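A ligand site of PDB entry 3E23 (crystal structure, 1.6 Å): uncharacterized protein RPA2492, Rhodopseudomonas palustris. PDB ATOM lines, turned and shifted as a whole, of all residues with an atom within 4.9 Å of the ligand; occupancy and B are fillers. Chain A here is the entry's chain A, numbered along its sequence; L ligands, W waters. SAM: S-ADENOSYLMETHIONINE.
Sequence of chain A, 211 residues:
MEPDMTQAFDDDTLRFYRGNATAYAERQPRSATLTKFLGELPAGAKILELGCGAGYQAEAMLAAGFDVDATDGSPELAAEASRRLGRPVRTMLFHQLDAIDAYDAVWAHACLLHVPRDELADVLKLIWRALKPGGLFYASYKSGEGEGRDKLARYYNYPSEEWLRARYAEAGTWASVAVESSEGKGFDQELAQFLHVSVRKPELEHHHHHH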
ATOM      1  N   ALA A   8      -1.749 -16.542  36.429  1.00  0.00           N
ATOM      2  CA  ALA A   8      -2.302 -17.809  35.979  1.00  0.00           C
ATOM      3  C   ALA A   8      -2.814 -17.766  34.544  1.00  0.00           C
ATOM      4  O   ALA A   8      -3.527 -18.670  34.113  1.00  0.00           O
ATOM      5  CB  ALA A   8      -3.437 -18.235  36.919  1.00  0.00           C
ATOM      6  N   PHE A   9      -2.449 -16.715  33.809  1.00  0.00           N
ATOM      7  CA  PHE A   9      -2.868 -16.612  32.426  1.00  0.00           C
ATOM      8  C   PHE A   9      -1.785 -15.936  31.595  1.00  0.00           C
ATOM      9  O   PHE A   9      -0.962 -15.196  32.122  1.00  0.00           O
ATOM     10  CB  PHE A   9      -4.186 -15.842  32.299  1.00  0.00           C
ATOM     11  CG  PHE A   9      -4.088 -14.386  32.695  1.00  0.00           C
ATOM     12  CD1 PHE A   9      -3.986 -14.026  34.026  1.00  0.00           C
ATOM     13  CD2 PHE A   9      -4.092 -13.392  31.724  1.00  0.00           C
ATOM     14  CE1 PHE A   9      -3.895 -12.681  34.393  1.00  0.00           C
ATOM     15  CE2 PHE A   9      -4.004 -12.047  32.077  1.00  0.00           C
ATOM     16  CZ  PHE A   9      -3.900 -11.697  33.421  1.00  0.00           C
ATOM     17  N   THR A  13      -1.618 -14.975  24.631  1.00  0.00           N
ATOM     18  CA  THR A  13      -2.509 -16.048  24.224  1.00  0.00           C
ATOM     19  C   THR A  13      -3.927 -15.465  24.147  1.00  0.00           C
ATOM     20  O   THR A  13      -4.626 -15.654  23.149  1.00  0.00           O
ATOM     21  CB  THR A  13      -2.488 -17.204  25.233  1.00  0.00           C
ATOM     22  OG1 THR A  13      -1.178 -17.794  25.255  1.00  0.00           O
ATOM     23  CG2 THR A  13      -3.509 -18.270  24.863  1.00  0.00           C
ATOM     24  N   LEU A  14      -4.335 -14.742  25.184  1.00  0.00           N
ATOM     25  CA  LEU A  14      -5.664 -14.150  25.174  1.00  0.00           C
ATOM     26  C   LEU A  14      -5.793 -13.102  24.071  1.00  0.00           C
ATOM     27  O   LEU A  14      -6.846 -12.968  23.449  1.00  0.00           O
ATOM     28  CB  LEU A  14      -5.980 -13.524  26.537  1.00  0.00           C
ATOM     29  CG  LEU A  14      -6.381 -14.556  27.615  1.00  0.00           C
ATOM     30  CD1 LEU A  14      -6.343 -13.915  28.985  1.00  0.00           C
ATOM     31  CD2 LEU A  14      -7.774 -15.089  27.292  1.00  0.00           C
ATOM     32  N   TYR A  17      -6.784 -14.652  20.679  1.00  0.00           N
ATOM     33  CA  TYR A  17      -8.193 -14.989  20.529  1.00  0.00           C
ATOM     34  C   TYR A  17      -9.083 -13.759  20.377  1.00  0.00           C
ATOM     35  O   TYR A  17     -10.128 -13.828  19.743  1.00  0.00           O
ATOM     36  CB  TYR A  17      -8.636 -15.852  21.706  1.00  0.00           C
ATOM     37  CG  TYR A  17      -8.001 -17.224  21.688  1.00  0.00           C
ATOM     38  CD1 TYR A  17      -8.362 -18.160  20.735  1.00  0.00           C
ATOM     39  CD2 TYR A  17      -7.014 -17.567  22.620  1.00  0.00           C
ATOM     40  CE1 TYR A  17      -7.766 -19.426  20.707  1.00  0.00           C
ATOM     41  CE2 TYR A  17      -6.417 -18.822  22.592  1.00  0.00           C
ATOM     42  CZ  TYR A  17      -6.794 -19.747  21.628  1.00  0.00           C
ATOM     43  OH  TYR A  17      -6.212 -20.991  21.588  1.00  0.00           O
ATOM     44  N   TYR A  24     -11.292 -17.899  14.151  1.00  0.00           N
ATOM     45  CA  TYR A  24     -11.259 -19.028  15.071  1.00  0.00           C
ATOM     46  C   TYR A  24     -12.627 -19.636  15.351  1.00  0.00           C
ATOM     47  O   TYR A  24     -12.753 -20.858  15.530  1.00  0.00           O
ATOM     48  CB  TYR A  24     -10.592 -18.619  16.383  1.00  0.00           C
ATOM     49  CG  TYR A  24     -10.411 -19.797  17.305  1.00  0.00           C
ATOM     50  CD1 TYR A  24     -11.403 -20.141  18.221  1.00  0.00           C
ATOM     51  CD2 TYR A  24      -9.295 -20.627  17.194  1.00  0.00           C
ATOM     52  CE1 TYR A  24     -11.298 -21.292  18.987  1.00  0.00           C
ATOM     53  CE2 TYR A  24      -9.186 -21.788  17.951  1.00  0.00           C
ATOM     54  CZ  TYR A  24     -10.195 -22.110  18.842  1.00  0.00           C
ATOM     55  OH  TYR A  24     -10.114 -23.268  19.570  1.00  0.00           O
ATOM     56  N   PRO A  29     -14.739 -28.041  17.123  1.00  0.00           N
ATOM     57  CA  PRO A  29     -13.917 -29.084  17.735  1.00  0.00           C
ATOM     58  C   PRO A  29     -14.514 -30.473  17.518  1.00  0.00           C
ATOM     59  O   PRO A  29     -15.711 -30.618  17.222  1.00  0.00           O
ATOM     60  CB  PRO A  29     -13.901 -28.680  19.209  1.00  0.00           C
ATOM     61  CG  PRO A  29     -15.245 -28.053  19.398  1.00  0.00           C
ATOM     62  CD  PRO A  29     -15.408 -27.215  18.141  1.00  0.00           C
ATOM     63  N   GLU A  49     -18.402 -25.060  31.892  1.00  0.00           N
ATOM     64  CA  GLU A  49     -17.464 -25.186  30.786  1.00  0.00           C
ATOM     65  C   GLU A  49     -16.471 -24.041  30.895  1.00  0.00           C
ATOM     66  O   GLU A  49     -16.860 -22.881  30.992  1.00  0.00           O
ATOM     67  CB  GLU A  49     -18.107 -25.146  29.388  1.00  0.00           C
ATOM     68  CG  GLU A  49     -17.018 -25.070  28.287  1.00  0.00           C
ATOM     69  CD  GLU A  49     -17.486 -25.415  26.880  1.00  0.00           C
ATOM     70  OE1 GLU A  49     -18.668 -25.209  26.548  1.00  0.00           O
ATOM     71  OE2 GLU A  49     -16.632 -25.888  26.086  1.00  0.00           O
ATOM     72  N   LEU A  50     -15.195 -24.394  30.921  1.00  0.00           N
ATOM     73  CA  LEU A  50     -14.123 -23.410  30.989  1.00  0.00           C
ATOM     74  C   LEU A  50     -13.602 -23.256  29.561  1.00  0.00           C
ATOM     75  O   LEU A  50     -13.618 -24.214  28.790  1.00  0.00           O
ATOM     76  CB  LEU A  50     -12.995 -23.913  31.894  1.00  0.00           C
ATOM     77  CG  LEU A  50     -13.363 -24.085  33.360  1.00  0.00           C
ATOM     78  CD1 LEU A  50     -12.206 -24.725  34.119  1.00  0.00           C
ATOM     79  CD2 LEU A  50     -13.715 -22.731  33.958  1.00  0.00           C
ATOM     80  N   GLY A  51     -13.141 -22.050  29.226  1.00  0.00           N
ATOM     81  CA  GLY A  51     -12.612 -21.784  27.899  1.00  0.00           C
ATOM     82  C   GLY A  51     -13.453 -22.370  26.791  1.00  0.00           C
ATOM     83  O   GLY A  51     -12.948 -23.063  25.906  1.00  0.00           O
ATOM     84  N   CYS A  52     -14.752 -22.083  26.828  1.00  0.00           N
ATOM     85  CA  CYS A  52     -15.703 -22.613  25.847  1.00  0.00           C
ATOM     86  C   CYS A  52     -15.503 -22.177  24.393  1.00  0.00           C
ATOM     87  O   CYS A  52     -16.131 -22.736  23.498  1.00  0.00           O
ATOM     88  CB  CYS A  52     -17.133 -22.263  26.269  1.00  0.00           C
ATOM     89  SG  CYS A  52     -17.562 -20.507  26.107  1.00  0.00           S
ATOM     90  N   GLY A  53     -14.644 -21.190  24.161  1.00  0.00           N
ATOM     91  CA  GLY A  53     -14.411 -20.737  22.810  1.00  0.00           C
ATOM     92  C   GLY A  53     -15.673 -20.214  22.138  1.00  0.00           C
ATOM     93  O   GLY A  53     -16.410 -19.416  22.714  1.00  0.00           O
ATOM     94  N   GLN A  57     -19.558 -26.733  21.726  1.00  0.00           N
ATOM     95  CA  GLN A  57     -19.814 -27.826  22.640  1.00  0.00           C
ATOM     96  C   GLN A  57     -20.858 -27.475  23.693  1.00  0.00           C
ATOM     97  O   GLN A  57     -21.637 -28.338  24.104  1.00  0.00           O
ATOM     98  CB  GLN A  57     -18.493 -28.297  23.248  1.00  0.00           C
ATOM     99  CG  GLN A  57     -17.518 -28.700  22.145  1.00  0.00           C
ATOM    100  CD  GLN A  57     -16.315 -29.470  22.638  1.00  0.00           C
ATOM    101  OE1 GLN A  57     -15.550 -28.990  23.472  1.00  0.00           O
ATOM    102  NE2 GLN A  57     -16.135 -30.671  22.095  1.00  0.00           N
ATOM    103  N   ASP A  72     -15.647 -18.224  29.156  1.00  0.00           N
ATOM    104  CA  ASP A  72     -14.402 -18.152  28.389  1.00  0.00           C
ATOM    105  C   ASP A  72     -13.633 -16.932  28.848  1.00  0.00           C
ATOM    106  O   ASP A  72     -14.218 -15.953  29.312  1.00  0.00           O
ATOM    107  CB  ASP A  72     -14.662 -18.071  26.883  1.00  0.00           C
ATOM    108  CG  ASP A  72     -13.402 -18.315  26.072  1.00  0.00           C
ATOM    109  OD1 ASP A  72     -12.708 -17.340  25.703  1.00  0.00           O
ATOM    110  OD2 ASP A  72     -13.081 -19.499  25.817  1.00  0.00           O
ATOM    111  N   GLY A  73     -12.310 -16.991  28.721  1.00  0.00           N
ATOM    112  CA  GLY A  73     -11.489 -15.879  29.152  1.00  0.00           C
ATOM    113  C   GLY A  73     -11.472 -14.717  28.178  1.00  0.00           C
ATOM    114  O   GLY A  73     -11.115 -13.597  28.554  1.00  0.00           O
ATOM    115  N   SER A  74     -11.864 -14.978  26.929  1.00  0.00           N
ATOM    116  CA  SER A  74     -11.885 -13.933  25.918  1.00  0.00           C
ATOM    117  C   SER A  74     -13.258 -13.307  25.759  1.00  0.00           C
ATOM    118  O   SER A  74     -14.211 -13.978  25.393  1.00  0.00           O
ATOM    119  CB  SER A  74     -11.457 -14.502  24.559  1.00  0.00           C
ATOM    120  OG  SER A  74     -11.666 -13.564  23.524  1.00  0.00           O
ATOM    121  N   LEU A  77     -14.563 -13.932  22.188  1.00  0.00           N
ATOM    122  CA  LEU A  77     -15.066 -15.274  21.907  1.00  0.00           C
ATOM    123  C   LEU A  77     -16.343 -15.533  22.708  1.00  0.00           C
ATOM    124  O   LEU A  77     -17.271 -16.178  22.213  1.00  0.00           O
ATOM    125  CB  LEU A  77     -14.012 -16.330  22.227  1.00  0.00           C
ATOM    126  CG  LEU A  77     -12.990 -16.558  21.101  1.00  0.00           C
ATOM    127  CD1 LEU A  77     -11.981 -17.608  21.511  1.00  0.00           C
ATOM    128  CD2 LEU A  77     -13.723 -16.989  19.833  1.00  0.00           C
ATOM    129  N   MET A  92     -14.671 -15.128  32.014  1.00  0.00           N
ATOM    130  CA  MET A  92     -14.019 -15.545  33.253  1.00  0.00           C
ATOM    131  C   MET A  92     -12.726 -16.268  32.958  1.00  0.00           C
ATOM    132  O   MET A  92     -12.688 -17.213  32.161  1.00  0.00           O
ATOM    133  CB  MET A  92     -14.954 -16.473  34.047  1.00  0.00           C
ATOM    134  CG  MET A  92     -14.404 -16.884  35.410  1.00  0.00           C
ATOM    135  SD  MET A  92     -15.444 -18.250  36.345  1.00  0.00           S
ATOM    136  CE  MET A  92     -14.727 -19.826  35.488  1.00  0.00           C
ATOM    137  N   LEU A  93     -11.646 -15.821  33.589  1.00  0.00           N
ATOM    138  CA  LEU A  93     -10.347 -16.463  33.432  1.00  0.00           C
ATOM    139  C   LEU A  93     -10.370 -17.645  34.393  1.00  0.00           C
ATOM    140  O   LEU A  93     -11.043 -17.594  35.423  1.00  0.00           O
ATOM    141  CB  LEU A  93      -9.230 -15.490  33.801  1.00  0.00           C
ATOM    142  CG  LEU A  93      -9.112 -14.310  32.840  1.00  0.00           C
ATOM    143  CD1 LEU A  93      -8.136 -13.276  33.387  1.00  0.00           C
ATOM    144  CD2 LEU A  93      -8.654 -14.792  31.469  1.00  0.00           C
ATOM    145  N   PHE A  94      -9.647 -18.709  34.070  1.00  0.00           N
ATOM    146  CA  PHE A  94      -9.633 -19.908  34.913  1.00  0.00           C
ATOM    147  C   PHE A  94      -9.406 -19.622  36.388  1.00  0.00           C
ATOM    148  O   PHE A  94     -10.146 -20.109  37.238  1.00  0.00           O
ATOM    149  CB  PHE A  94      -8.551 -20.889  34.452  1.00  0.00           C
ATOM    150  CG  PHE A  94      -8.608 -21.247  32.996  1.00  0.00           C
ATOM    151  CD1 PHE A  94      -9.811 -21.638  32.400  1.00  0.00           C
ATOM    152  CD2 PHE A  94      -7.458 -21.224  32.221  1.00  0.00           C
ATOM    153  CE1 PHE A  94      -9.857 -21.995  31.057  1.00  0.00           C
ATOM    154  CE2 PHE A  94      -7.499 -21.582  30.870  1.00  0.00           C
ATOM    155  CZ  PHE A  94      -8.699 -21.973  30.288  1.00  0.00           C
ATOM    156  N   HIS A 109     -12.183 -28.270  27.338  1.00  0.00           N
ATOM    157  CA  HIS A 109     -11.586 -28.788  26.115  1.00  0.00           C
ATOM    158  C   HIS A 109     -10.524 -27.863  25.532  1.00  0.00           C
ATOM    159  O   HIS A 109     -10.803 -26.714  25.190  1.00  0.00           O
ATOM    160  CB  HIS A 109     -12.685 -29.057  25.077  1.00  0.00           C
ATOM    161  CG  HIS A 109     -12.219 -29.840  23.881  1.00  0.00           C
ATOM    162  ND1 HIS A 109     -12.024 -29.269  22.648  1.00  0.00           N
ATOM    163  CD2 HIS A 109     -11.949 -31.157  23.737  1.00  0.00           C
ATOM    164  CE1 HIS A 109     -11.648 -30.207  21.789  1.00  0.00           C
ATOM    165  NE2 HIS A 109     -11.589 -31.365  22.420  1.00  0.00           N
ATOM    166  N   ALA A 110      -9.306 -28.382  25.431  1.00  0.00           N
ATOM    167  CA  ALA A 110      -8.171 -27.658  24.864  1.00  0.00           C
ATOM    168  C   ALA A 110      -8.026 -26.218  25.315  1.00  0.00           C
ATOM    169  O   ALA A 110      -7.862 -25.314  24.492  1.00  0.00           O
ATOM    170  CB  ALA A 110      -8.248 -27.722  23.344  1.00  0.00           C
ATOM    171  N   CYS A 111      -8.079 -25.990  26.620  1.00  0.00           N
ATOM    172  CA  CYS A 111      -7.954 -24.627  27.125  1.00  0.00           C
ATOM    173  C   CYS A 111      -7.028 -24.514  28.331  1.00  0.00           C
ATOM    174  O   CYS A 111      -6.306 -23.525  28.463  1.00  0.00           O
ATOM    175  CB  CYS A 111      -9.339 -24.062  27.461  1.00  0.00           C
ATOM    176  SG  CYS A 111     -10.239 -24.967  28.711  1.00  0.00           S
ATOM    177  N   HIS A 114      -3.304 -23.679  28.152  1.00  0.00           N
ATOM    178  CA  HIS A 114      -2.813 -22.302  28.044  1.00  0.00           C
ATOM    179  C   HIS A 114      -2.434 -21.734  29.409  1.00  0.00           C
ATOM    180  O   HIS A 114      -2.099 -20.555  29.530  1.00  0.00           O
ATOM    181  CB  HIS A 114      -3.876 -21.411  27.391  1.00  0.00           C
ATOM    182  CG  HIS A 114      -3.995 -21.590  25.914  1.00  0.00           C
ATOM    183  ND1 HIS A 114      -5.194 -21.538  25.244  1.00  0.00           N
ATOM    184  CD2 HIS A 114      -3.048 -21.805  24.965  1.00  0.00           C
ATOM    185  CE1 HIS A 114      -4.988 -21.725  23.948  1.00  0.00           C
ATOM    186  NE2 HIS A 114      -3.693 -21.883  23.754  1.00  0.00           N
ATOM    187  N   ARG A 154       0.665 -18.166  20.859  1.00  0.00           N
ATOM    188  CA  ARG A 154      -0.103 -18.829  21.909  1.00  0.00           C
ATOM    189  C   ARG A 154       0.790 -19.716  22.775  1.00  0.00           C
ATOM    190  O   ARG A 154       1.547 -20.545  22.274  1.00  0.00           O
ATOM    191  CB  ARG A 154      -1.197 -19.697  21.297  1.00  0.00           C
ATOM    192  CG  ARG A 154      -2.238 -18.932  20.491  1.00  0.00           C
ATOM    193  CD  ARG A 154      -3.359 -19.855  20.080  1.00  0.00           C
ATOM    194  NE  ARG A 154      -2.884 -20.936  19.226  1.00  0.00           N
ATOM    195  CZ  ARG A 154      -3.630 -21.947  18.808  1.00  0.00           C
ATOM    196  NH1 ARG A 154      -4.908 -22.031  19.155  1.00  0.00           N
ATOM    197  NH2 ARG A 154      -3.097 -22.873  18.023  1.00  0.00           N
HETATM  198  N   SAM L   1     -13.060 -25.355  24.102  1.00  0.00           N
HETATM  199  CA  SAM L   1     -12.764 -24.778  22.731  1.00  0.00           C
HETATM  200  C   SAM L   1     -12.584 -25.627  21.504  1.00  0.00           C
HETATM  201  O   SAM L   1     -12.897 -25.211  20.406  1.00  0.00           O
HETATM  202  OXT SAM L   1     -12.147 -26.789  21.650  1.00  0.00           O
HETATM  203  CB  SAM L   1     -11.882 -23.471  22.577  1.00  0.00           C
HETATM  204  CG  SAM L   1     -10.386 -23.934  22.573  1.00  0.00           C
HETATM  205  SD  SAM L   1      -9.204 -22.605  22.345  1.00  0.00           S
HETATM  206  CE  SAM L   1      -7.863 -23.621  21.789  1.00  0.00           C
HETATM  207  C5' SAM L   1      -8.387 -22.152  23.841  1.00  0.00           C
HETATM  208  C4' SAM L   1      -9.592 -21.421  24.711  1.00  0.00           C
HETATM  209  O4' SAM L   1      -9.043 -21.148  26.033  1.00  0.00           O
HETATM  210  C3' SAM L   1     -10.025 -20.046  23.979  1.00  0.00           C
HETATM  211  O3' SAM L   1     -11.418 -19.863  23.732  1.00  0.00           O
HETATM  212  C2' SAM L   1      -9.399 -18.973  24.860  1.00  0.00           C
HETATM  213  O2' SAM L   1     -10.188 -17.724  24.852  1.00  0.00           O
HETATM  214  C1' SAM L   1      -9.474 -19.647  26.296  1.00  0.00           C
HETATM  215  N9  SAM L   1      -8.603 -18.900  26.994  1.00  0.00           N
HETATM  216  C8  SAM L   1      -7.242 -18.704  26.761  1.00  0.00           C
HETATM  217  N7  SAM L   1      -6.693 -18.381  28.018  1.00  0.00           N
HETATM  218  C5  SAM L   1      -7.580 -18.556  29.007  1.00  0.00           C
HETATM  219  C6  SAM L   1      -7.628 -18.255  30.450  1.00  0.00           C
HETATM  220  N6  SAM L   1      -6.531 -17.993  31.039  1.00  0.00           N
HETATM  221  N1  SAM L   1      -8.830 -18.244  31.071  1.00  0.00           N
HETATM  222  C2  SAM L   1      -9.893 -18.704  30.428  1.00  0.00           C
HETATM  223  N3  SAM L   1     -10.018 -18.789  29.092  1.00  0.00           N
HETATM  224  C4  SAM L   1      -8.894 -18.763  28.301  1.00  0.00           C
HETATM  225  O   HOH W   1     -10.018 -27.376  20.102  1.00  0.00           O
HETATM  226  O   HOH W   2      -6.431 -18.007  34.178  1.00  0.00           O
HETATM  227  O   HOH W   3     -15.514 -26.249  23.696  1.00  0.00           O
HETATM  228  O   HOH W   4     -13.944 -26.138  26.829  1.00  0.00           O
HETATM  229  O   HOH W   5     -14.489 -22.989  19.911  1.00  0.00           O
HETATM  230  O   HOH W   6     -12.265 -25.673  17.864  1.00  0.00           O
HETATM  231  O   HOH W   7      -3.928 -18.185  29.548  1.00  0.00           O
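A nitrogen (N) of the ligand lies within hydrogen-bond range of the backbone carbonyl oxygen (O) of His 109 (2.9 Å). An oxygen (OXT) of the ligand lies within hydrogen-bond range of a ring nitrogen (ND1) of His 109 (2.7 Å). An oxygen (O2') of the ligand is in hydrogen-bond range of the side-chain carboxylate of Asp 72 (2.7 Å). The backbone carbonyl oxygen (O) of Gly 51 sits at hydrogen-bond distance from a nitrogen (N) of the ligand (2.9 Å). N of Gly 73 lies within hydrogen-bond range of N3 of the ligand (2.9 Å). An oxygen (O) of the ligand sits close to the side-chain hydroxyl (OH) of Tyr 24, at 3.5 Å. N1 of the ligand is in hydrogen-bond range of N of Phe 94 (3.1 Å).
The backbone NH (N) of Gly 53 sits at hydrogen-bond distance from the side-chain carboxylate (OD2) of Asp 72, 2.8 Å away. The side-chain carboxylate of Asp 72 is in hydrogen-bond range of the backbone NH of Ser 74, 2.8 Å away. The backbone carbonyl oxygen (O) of Asp 72 lies within hydrogen-bond range of the backbone NH (N) of Met 92 (2.9 Å). The backbone NH of Cys 52 is in hydrogen-bond range of the side-chain carboxylate of Asp 72, 3.2 Å away. The backbone NH (N) of Gly 73 sits at hydrogen-bond distance from the backbone carbonyl oxygen (O) of Met 92 (3.5 Å). OH of Tyr 17 is in hydrogen-bond range of NH1 of Arg 154 (2.9 Å). The side-chain hydroxyl (OG) of Ser 74 lies within hydrogen-bond range of the backbone NH (N) of Leu 77, 3.2 Å away. The backbone carbonyl oxygen of Leu 50 lies within hydrogen-bond range of the side-chain sulfur of Cys 111 (3.5 Å).
OH of Tyr 17 lies close to SD of the ligand, at 3.5 Å. A sulfur (SD) of the ligand sits close to the backbone carbonyl oxygen of Ala 110 (3.7 Å). CB of Phe 9 touches N6 of the ligand, at 3.4 Å. Leu 14 touches the ligand (CD2 to N7, 3.5 Å). CB of Pro 29 touches OXT of the ligand, 3.6 Å away. CA of Gly 53 touches O3' of the ligand, 3.3 Å away. CB of Ser 74 touches O2' of the ligand, 3.5 Å away. Leu 77 touches the ligand (CD1 to O3', 3.2 Å). Met 92 touches the ligand (O to C2, 3.6 Å). Leu 93 touches the ligand. Cys 111 touches the ligand. His 114 touches the ligand. Hydrophobic or aromatic side chains that line the ligand: Phe 9, Leu 14, Tyr 17, Tyr 24, Pro 29, Leu 77, Leu 93, Phe 94, His 109 and His 114. 18 residues have an atom within 4 Å of the ligand: Phe 9, Leu 14, Tyr 17, Tyr 24, Pro 29, Gly 51, Gly 53, Asp 72, Gly 73, Ser 74, Leu 77, Met 92, Leu 93, Phe 94, His 109, Ala 110, Cys 111 and His 114.
Water W3 lies within hydrogen-bond range of a nitrogen (N) of the ligand (2.6 Å), the side-chain carboxylate of Glu 49 (2.7 Å) and the side-chain amide oxygen of Gln 57 (2.8 Å). Water W7 bridges the backbone carbonyl oxygen of His 114 and a nitrogen (N6) of the ligand. Water W2 lies within hydrogen-bond range of O of Ala 8, N6 of the ligand and N of Phe 94.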
